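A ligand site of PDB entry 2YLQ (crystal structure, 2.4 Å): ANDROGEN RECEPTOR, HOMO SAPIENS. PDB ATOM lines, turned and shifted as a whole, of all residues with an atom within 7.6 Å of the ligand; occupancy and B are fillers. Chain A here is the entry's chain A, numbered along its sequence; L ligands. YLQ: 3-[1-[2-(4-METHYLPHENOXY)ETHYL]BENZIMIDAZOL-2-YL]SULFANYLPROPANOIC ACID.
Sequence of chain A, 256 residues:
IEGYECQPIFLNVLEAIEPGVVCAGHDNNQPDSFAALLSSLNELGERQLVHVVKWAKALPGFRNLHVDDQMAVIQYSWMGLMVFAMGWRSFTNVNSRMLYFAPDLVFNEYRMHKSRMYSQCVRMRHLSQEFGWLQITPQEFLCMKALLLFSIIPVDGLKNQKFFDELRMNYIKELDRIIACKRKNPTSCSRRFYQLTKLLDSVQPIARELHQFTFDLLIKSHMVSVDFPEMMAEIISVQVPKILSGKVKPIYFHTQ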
ATOM      1  N   PHE A  10      11.143 -32.100 -17.257  1.00  0.00           N
ATOM      2  CA  PHE A  10      11.202 -30.987 -18.245  1.00  0.00           C
ATOM      3  C   PHE A  10      10.258 -29.783 -17.919  1.00  0.00           C
ATOM      4  O   PHE A  10      10.665 -28.631 -18.008  1.00  0.00           O
ATOM      5  CB  PHE A  10      10.963 -31.520 -19.654  1.00  0.00           C
ATOM      6  CG  PHE A  10      10.874 -30.451 -20.694  1.00  0.00           C
ATOM      7  CD1 PHE A  10      12.040 -29.877 -21.221  1.00  0.00           C
ATOM      8  CD2 PHE A  10       9.621 -30.044 -21.199  1.00  0.00           C
ATOM      9  CE1 PHE A  10      11.963 -28.880 -22.236  1.00  0.00           C
ATOM     10  CE2 PHE A  10       9.511 -29.046 -22.190  1.00  0.00           C
ATOM     11  CZ  PHE A  10      10.692 -28.459 -22.713  1.00  0.00           C
ATOM     12  N   LEU A  59      17.376 -22.727 -20.108  1.00  0.00           N
ATOM     13  CA  LEU A  59      16.495 -23.738 -20.669  1.00  0.00           C
ATOM     14  C   LEU A  59      17.269 -25.066 -20.820  1.00  0.00           C
ATOM     15  O   LEU A  59      18.460 -25.069 -21.035  1.00  0.00           O
ATOM     16  CB  LEU A  59      15.894 -23.318 -21.999  1.00  0.00           C
ATOM     17  CG  LEU A  59      14.640 -22.456 -21.929  1.00  0.00           C
ATOM     18  CD1 LEU A  59      14.590 -21.672 -23.222  1.00  0.00           C
ATOM     19  CD2 LEU A  59      13.269 -23.247 -21.648  1.00  0.00           C
ATOM     20  N   PRO A  60      16.579 -26.201 -20.720  1.00  0.00           N
ATOM     21  CA  PRO A  60      17.350 -27.436 -20.952  1.00  0.00           C
ATOM     22  C   PRO A  60      18.041 -27.560 -22.338  1.00  0.00           C
ATOM     23  O   PRO A  60      17.392 -27.420 -23.366  1.00  0.00           O
ATOM     24  CB  PRO A  60      16.279 -28.546 -20.747  1.00  0.00           C
ATOM     25  CG  PRO A  60      15.291 -27.933 -19.767  1.00  0.00           C
ATOM     26  CD  PRO A  60      15.221 -26.469 -20.182  1.00  0.00           C
ATOM     27  N   GLY A  61      19.356 -27.795 -22.350  1.00  0.00           N
ATOM     28  CA  GLY A  61      20.094 -28.018 -23.605  1.00  0.00           C
ATOM     29  C   GLY A  61      20.656 -26.768 -24.276  1.00  0.00           C
ATOM     30  O   GLY A  61      21.541 -26.862 -25.144  1.00  0.00           O
ATOM     31  N   PHE A  62      20.195 -25.593 -23.826  1.00  0.00           N
ATOM     32  CA  PHE A  62      20.508 -24.357 -24.511  1.00  0.00           C
ATOM     33  C   PHE A  62      21.989 -24.032 -24.550  1.00  0.00           C
ATOM     34  O   PHE A  62      22.463 -23.436 -25.535  1.00  0.00           O
ATOM     35  CB  PHE A  62      19.722 -23.188 -23.927  1.00  0.00           C
ATOM     36  CG  PHE A  62      19.882 -21.902 -24.692  1.00  0.00           C
ATOM     37  CD1 PHE A  62      19.146 -21.654 -25.824  1.00  0.00           C
ATOM     38  CD2 PHE A  62      20.773 -20.921 -24.272  1.00  0.00           C
ATOM     39  CE1 PHE A  62      19.277 -20.462 -26.538  1.00  0.00           C
ATOM     40  CE2 PHE A  62      20.892 -19.726 -24.951  1.00  0.00           C
ATOM     41  CZ  PHE A  62      20.147 -19.494 -26.100  1.00  0.00           C
ATOM     42  N   ARG A  63      22.732 -24.344 -23.486  1.00  0.00           N
ATOM     43  CA  ARG A  63      24.164 -23.936 -23.458  1.00  0.00           C
ATOM     44  C   ARG A  63      25.059 -24.847 -24.355  1.00  0.00           C
ATOM     45  O   ARG A  63      26.195 -24.478 -24.680  1.00  0.00           O
ATOM     46  CB  ARG A  63      24.724 -23.859 -22.029  1.00  0.00           C
ATOM     47  CG  ARG A  63      23.799 -23.258 -20.950  1.00  0.00           C
ATOM     48  CD  ARG A  63      24.227 -21.834 -20.429  1.00  0.00           C
ATOM     49  NE  ARG A  63      25.490 -21.796 -19.665  1.00  0.00           N
ATOM     50  CZ  ARG A  63      25.952 -20.713 -19.053  1.00  0.00           C
ATOM     51  NH1 ARG A  63      25.264 -19.575 -19.078  1.00  0.00           N
ATOM     52  NH2 ARG A  63      27.104 -20.746 -18.397  1.00  0.00           N
ATOM     53  N   ASN A  64      24.534 -26.034 -24.703  1.00  0.00           N
ATOM     54  CA  ASN A  64      25.014 -26.922 -25.763  1.00  0.00           C
ATOM     55  C   ASN A  64      25.197 -26.238 -27.118  1.00  0.00           C
ATOM     56  O   ASN A  64      26.029 -26.662 -27.908  1.00  0.00           O
ATOM     57  CB  ASN A  64      24.006 -28.069 -26.026  1.00  0.00           C
ATOM     58  CG  ASN A  64      24.086 -29.207 -24.980  1.00  0.00           C
ATOM     59  OD1 ASN A  64      24.939 -29.183 -24.082  1.00  0.00           O
ATOM     60  ND2 ASN A  64      23.180 -30.202 -25.105  1.00  0.00           N
ATOM     61  N   LEU A  65      24.375 -25.245 -27.428  1.00  0.00           N
ATOM     62  CA  LEU A  65      24.518 -24.536 -28.664  1.00  0.00           C
ATOM     63  C   LEU A  65      25.792 -23.737 -28.614  1.00  0.00           C
ATOM     64  O   LEU A  65      26.190 -23.242 -27.530  1.00  0.00           O
ATOM     65  CB  LEU A  65      23.366 -23.567 -28.912  1.00  0.00           C
ATOM     66  CG  LEU A  65      21.932 -24.043 -29.021  1.00  0.00           C
ATOM     67  CD1 LEU A  65      21.027 -22.801 -29.155  1.00  0.00           C
ATOM     68  CD2 LEU A  65      21.719 -25.062 -30.159  1.00  0.00           C
ATOM     69  N   ASN A 160      26.694 -23.882 -35.382  1.00  0.00           N
ATOM     70  CA  ASN A 160      26.410 -25.324 -35.251  1.00  0.00           C
ATOM     71  C   ASN A 160      24.930 -25.691 -35.379  1.00  0.00           C
ATOM     72  O   ASN A 160      24.206 -25.849 -34.381  1.00  0.00           O
ATOM     73  CB  ASN A 160      27.049 -25.993 -34.031  1.00  0.00           C
ATOM     74  CG  ASN A 160      26.980 -27.547 -34.106  1.00  0.00           C
ATOM     75  OD1 ASN A 160      26.721 -28.152 -35.166  1.00  0.00           O
ATOM     76  ND2 ASN A 160      27.223 -28.191 -32.973  1.00  0.00           N
ATOM     77  N   LYS A 162      23.640 -28.521 -36.542  1.00  0.00           N
ATOM     78  CA  LYS A 162      23.247 -29.901 -36.198  1.00  0.00           C
ATOM     79  C   LYS A 162      22.709 -29.943 -34.767  1.00  0.00           C
ATOM     80  O   LYS A 162      21.658 -30.566 -34.470  1.00  0.00           O
ATOM     81  CB  LYS A 162      24.375 -30.923 -36.442  1.00  0.00           C
ATOM     82  N   PHE A 163      23.414 -29.244 -33.877  1.00  0.00           N
ATOM     83  CA  PHE A 163      22.987 -29.103 -32.489  1.00  0.00           C
ATOM     84  C   PHE A 163      21.638 -28.361 -32.385  1.00  0.00           C
ATOM     85  O   PHE A 163      20.736 -28.770 -31.626  1.00  0.00           O
ATOM     86  CB  PHE A 163      24.086 -28.431 -31.641  1.00  0.00           C
ATOM     87  CG  PHE A 163      25.307 -29.338 -31.351  1.00  0.00           C
ATOM     88  CD1 PHE A 163      25.494 -30.573 -32.025  1.00  0.00           C
ATOM     89  CD2 PHE A 163      26.286 -28.954 -30.405  1.00  0.00           C
ATOM     90  CE1 PHE A 163      26.632 -31.402 -31.764  1.00  0.00           C
ATOM     91  CE2 PHE A 163      27.417 -29.773 -30.151  1.00  0.00           C
ATOM     92  CZ  PHE A 163      27.575 -31.003 -30.832  1.00  0.00           C
ATOM     93  N   PHE A 164      21.470 -27.260 -33.140  1.00  0.00           N
ATOM     94  CA  PHE A 164      20.179 -26.597 -33.156  1.00  0.00           C
ATOM     95  C   PHE A 164      19.033 -27.552 -33.596  1.00  0.00           C
ATOM     96  O   PHE A 164      17.944 -27.555 -32.947  1.00  0.00           O
ATOM     97  CB  PHE A 164      20.213 -25.326 -33.995  1.00  0.00           C
ATOM     98  CG  PHE A 164      18.891 -24.624 -34.070  1.00  0.00           C
ATOM     99  CD1 PHE A 164      17.880 -25.103 -34.901  1.00  0.00           C
ATOM    100  CD2 PHE A 164      18.650 -23.503 -33.287  1.00  0.00           C
ATOM    101  CE1 PHE A 164      16.635 -24.485 -34.948  1.00  0.00           C
ATOM    102  CE2 PHE A 164      17.387 -22.818 -33.328  1.00  0.00           C
ATOM    103  CZ  PHE A 164      16.367 -23.337 -34.153  1.00  0.00           C
ATOM    104  N   ASP A 165      19.271 -28.345 -34.637  1.00  0.00           N
ATOM    105  CA  ASP A 165      18.235 -29.287 -35.131  1.00  0.00           C
ATOM    106  C   ASP A 165      17.805 -30.350 -34.104  1.00  0.00           C
ATOM    107  O   ASP A 165      16.612 -30.612 -33.949  1.00  0.00           O
ATOM    108  CB  ASP A 165      18.613 -29.907 -36.489  1.00  0.00           C
ATOM    109  CG  ASP A 165      18.700 -28.857 -37.632  1.00  0.00           C
ATOM    110  OD1 ASP A 165      18.221 -27.692 -37.529  1.00  0.00           O
ATOM    111  OD2 ASP A 165      19.269 -29.215 -38.683  1.00  0.00           O
ATOM    112  N   GLU A 166      18.767 -30.940 -33.386  1.00  0.00           N
ATOM    113  CA  GLU A 166      18.427 -31.922 -32.353  1.00  0.00           C
ATOM    114  C   GLU A 166      17.675 -31.238 -31.187  1.00  0.00           C
ATOM    115  O   GLU A 166      16.681 -31.760 -30.671  1.00  0.00           O
ATOM    116  CB  GLU A 166      19.673 -32.705 -31.898  1.00  0.00           C
ATOM    117  CG  GLU A 166      19.801 -33.030 -30.388  1.00  0.00           C
ATOM    118  CD  GLU A 166      20.291 -34.455 -30.077  1.00  0.00           C
ATOM    119  OE1 GLU A 166      19.776 -35.421 -30.705  1.00  0.00           O
ATOM    120  OE2 GLU A 166      21.143 -34.607 -29.172  1.00  0.00           O
ATOM    121  N   LEU A 167      18.124 -30.058 -30.826  1.00  0.00           N
ATOM    122  CA  LEU A 167      17.531 -29.329 -29.748  1.00  0.00           C
ATOM    123  C   LEU A 167      16.075 -29.007 -30.071  1.00  0.00           C
ATOM    124  O   LEU A 167      15.149 -29.338 -29.312  1.00  0.00           O
ATOM    125  CB  LEU A 167      18.336 -28.072 -29.516  1.00  0.00           C
ATOM    126  CG  LEU A 167      18.063 -27.392 -28.194  1.00  0.00           C
ATOM    127  CD1 LEU A 167      17.986 -28.429 -27.026  1.00  0.00           C
ATOM    128  CD2 LEU A 167      19.070 -26.241 -27.940  1.00  0.00           C
ATOM    129  N   ARG A 168      15.869 -28.410 -31.246  1.00  0.00           N
ATOM    130  CA  ARG A 168      14.537 -28.052 -31.647  1.00  0.00           C
ATOM    131  C   ARG A 168      13.653 -29.320 -31.696  1.00  0.00           C
ATOM    132  O   ARG A 168      12.508 -29.309 -31.233  1.00  0.00           O
ATOM    133  CB  ARG A 168      14.548 -27.263 -32.984  1.00  0.00           C
ATOM    134  CG  ARG A 168      13.172 -27.169 -33.637  1.00  0.00           C
ATOM    135  CD  ARG A 168      13.180 -26.338 -34.947  1.00  0.00           C
ATOM    136  NE  ARG A 168      11.913 -26.565 -35.655  1.00  0.00           N
ATOM    137  CZ  ARG A 168      10.832 -25.805 -35.473  1.00  0.00           C
ATOM    138  NH1 ARG A 168      10.917 -24.770 -34.645  1.00  0.00           N
ATOM    139  NH2 ARG A 168       9.662 -26.065 -36.092  1.00  0.00           N
ATOM    140  N   MET A 169      14.181 -30.411 -32.257  1.00  0.00           N
ATOM    141  CA  MET A 169      13.403 -31.682 -32.302  1.00  0.00           C
ATOM    142  C   MET A 169      12.967 -32.095 -30.892  1.00  0.00           C
ATOM    143  O   MET A 169      11.832 -32.534 -30.701  1.00  0.00           O
ATOM    144  CB  MET A 169      14.206 -32.820 -32.949  1.00  0.00           C
ATOM    145  CG  MET A 169      13.671 -34.244 -32.681  1.00  0.00           C
ATOM    146  SD  MET A 169      14.778 -35.506 -33.479  1.00  0.00           S
ATOM    147  CE  MET A 169      16.275 -35.348 -32.477  1.00  0.00           C
ATOM    148  N   ASN A 170      13.867 -31.948 -29.905  1.00  0.00           N
ATOM    149  CA  ASN A 170      13.523 -32.318 -28.527  1.00  0.00           C
ATOM    150  C   ASN A 170      12.404 -31.447 -27.955  1.00  0.00           C
ATOM    151  O   ASN A 170      11.493 -31.964 -27.270  1.00  0.00           O
ATOM    152  CB  ASN A 170      14.752 -32.343 -27.592  1.00  0.00           C
ATOM    153  CG  ASN A 170      15.685 -33.551 -27.866  1.00  0.00           C
ATOM    154  OD1 ASN A 170      15.267 -34.560 -28.419  1.00  0.00           O
ATOM    155  ND2 ASN A 170      16.960 -33.419 -27.485  1.00  0.00           N
ATOM    156  N   TYR A 171      12.434 -30.137 -28.263  1.00  0.00           N
ATOM    157  CA  TYR A 171      11.343 -29.281 -27.796  1.00  0.00           C
ATOM    158  C   TYR A 171      10.012 -29.655 -28.407  1.00  0.00           C
ATOM    159  O   TYR A 171       8.990 -29.639 -27.723  1.00  0.00           O
ATOM    160  CB  TYR A 171      11.661 -27.810 -27.949  1.00  0.00           C
ATOM    161  CG  TYR A 171      12.555 -27.400 -26.817  1.00  0.00           C
ATOM    162  CD1 TYR A 171      13.917 -27.765 -26.796  1.00  0.00           C
ATOM    163  CD2 TYR A 171      12.047 -26.695 -25.731  1.00  0.00           C
ATOM    164  CE1 TYR A 171      14.762 -27.405 -25.723  1.00  0.00           C
ATOM    165  CE2 TYR A 171      12.870 -26.337 -24.668  1.00  0.00           C
ATOM    166  CZ  TYR A 171      14.238 -26.689 -24.664  1.00  0.00           C
ATOM    167  OH  TYR A 171      15.042 -26.310 -23.592  1.00  0.00           O
ATOM    168  N   LYS A 173       9.252 -32.692 -29.271  1.00  0.00           N
ATOM    169  CA  LYS A 173       8.891 -33.961 -28.650  1.00  0.00           C
ATOM    170  C   LYS A 173       8.220 -33.633 -27.325  1.00  0.00           C
ATOM    171  O   LYS A 173       7.204 -34.247 -26.940  1.00  0.00           O
ATOM    172  CB  LYS A 173      10.124 -34.852 -28.504  1.00  0.00           C
ATOM    173  N   GLU A 174       8.739 -32.584 -26.676  1.00  0.00           N
ATOM    174  CA  GLU A 174       8.255 -32.229 -25.340  1.00  0.00           C
ATOM    175  C   GLU A 174       6.826 -31.688 -25.311  1.00  0.00           C
ATOM    176  O   GLU A 174       6.047 -32.069 -24.450  1.00  0.00           O
ATOM    177  CB  GLU A 174       9.214 -31.303 -24.612  1.00  0.00           C
ATOM    178  CG  GLU A 174      10.497 -31.990 -24.099  1.00  0.00           C
ATOM    179  CD  GLU A 174      10.292 -33.334 -23.333  1.00  0.00           C
ATOM    180  OE1 GLU A 174       9.199 -33.608 -22.769  1.00  0.00           O
ATOM    181  OE2 GLU A 174      11.259 -34.121 -23.305  1.00  0.00           O
ATOM    182  N   ARG A 177       4.484 -34.521 -25.912  1.00  0.00           N
ATOM    183  CA  ARG A 177       4.295 -35.161 -24.572  1.00  0.00           C
ATOM    184  C   ARG A 177       3.218 -34.511 -23.670  1.00  0.00           C
ATOM    185  O   ARG A 177       2.324 -35.192 -23.135  1.00  0.00           O
ATOM    186  CB  ARG A 177       5.664 -35.223 -23.842  1.00  0.00           C
ATOM    187  CG  ARG A 177       5.640 -35.499 -22.315  1.00  0.00           C
ATOM    188  CD  ARG A 177       7.054 -35.783 -21.707  1.00  0.00           C
ATOM    189  NE  ARG A 177       7.479 -37.143 -22.044  1.00  0.00           N
ATOM    190  CZ  ARG A 177       8.340 -37.450 -23.005  1.00  0.00           C
ATOM    191  NH1 ARG A 177       8.922 -36.496 -23.718  1.00  0.00           N
ATOM    192  NH2 ARG A 177       8.635 -38.716 -23.246  1.00  0.00           N
HETATM  193  C01 YLQ L   1      14.812 -37.618 -29.565  1.00  0.00           C
HETATM  194  C02 YLQ L   1      15.674 -37.382 -28.369  1.00  0.00           C
HETATM  195  C03 YLQ L   1      15.144 -37.439 -27.116  1.00  0.00           C
HETATM  196  C04 YLQ L   1      16.001 -37.228 -25.974  1.00  0.00           C
HETATM  197  C05 YLQ L   1      17.385 -36.948 -26.154  1.00  0.00           C
HETATM  198  O06 YLQ L   1      18.195 -36.737 -25.083  1.00  0.00           O
HETATM  199  C07 YLQ L   1      17.875 -35.856 -24.057  1.00  0.00           C
HETATM  200  C08 YLQ L   1      18.608 -34.565 -24.055  1.00  0.00           C
HETATM  201  N09 YLQ L   1      17.898 -33.270 -24.286  1.00  0.00           N
HETATM  202  C10 YLQ L   1      18.426 -32.154 -24.857  1.00  0.00           C
HETATM  203  S11 YLQ L   1      20.022 -32.050 -25.526  1.00  0.00           S
HETATM  204  C12 YLQ L   1      19.711 -31.417 -27.208  1.00  0.00           C
HETATM  205  C13 YLQ L   1      20.731 -31.515 -28.268  1.00  0.00           C
HETATM  206  C14 YLQ L   1      21.877 -30.577 -28.318  1.00  0.00           C
HETATM  207  O15 YLQ L   1      22.072 -29.751 -27.405  1.00  0.00           O
HETATM  208  O16 YLQ L   1      22.684 -30.634 -29.308  1.00  0.00           O
HETATM  209  N17 YLQ L   1      17.525 -31.159 -24.884  1.00  0.00           N
HETATM  210  C18 YLQ L   1      16.388 -31.639 -24.311  1.00  0.00           C
HETATM  211  C19 YLQ L   1      15.141 -31.015 -24.076  1.00  0.00           C
HETATM  212  C20 YLQ L   1      14.165 -31.768 -23.458  1.00  0.00           C
HETATM  213  C21 YLQ L   1      14.389 -33.075 -23.065  1.00  0.00           C
HETATM  214  C22 YLQ L   1      15.622 -33.701 -23.290  1.00  0.00           C
HETATM  215  C23 YLQ L   1      16.619 -32.952 -23.922  1.00  0.00           C
HETATM  216  C24 YLQ L   1      17.913 -36.894 -27.439  1.00  0.00           C
HETATM  217  C25 YLQ L   1      17.087 -37.107 -28.542  1.00  0.00           C
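ND2 of Asn 64 lies within hydrogen-bond range of O15 of the ligand (2.6 Å). A nitrogen (N17) of the ligand sits close to the side-chain amide nitrogen (ND2) of Asn 170 (3.5 Å).
The side-chain carboxylate (OE1) of Glu 174 lies within salt-bridge range of the guanidinium group (NH1) of Arg 177 (3.1 Å). The backbone carbonyl oxygen of Pro 60 is in hydrogen-bond range of the side-chain hydroxyl of Tyr 171 (2.6 Å).
Residues that only touch the ligand: Glu 166 (2.8 Å), Glu 174 (3.3 Å), Leu 167 (3.5 Å), Phe 163 (3.5 Å), Phe 10 (3.6 Å), Gly 61 (3.7 Å), Met 169 (3.97 Å) and Tyr 171 (3.99 Å). Hydrophobic or aromatic side chains within 4 Å of the ligand: Phe 10, Phe 163, Leu 167, Met 169 and Tyr 171. Within 4 Å of the ligand: Phe 10, Gly 61, Asn 64, Phe 163, Glu 166, Leu 167, Met 169, Asn 170, Tyr 171 and Glu 174. Along chain A the residues within 4 Å of the ligand span positions 10 to 174. The nearest printed residue that does not touch the ligand is Pro 60 (4.04 Å).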
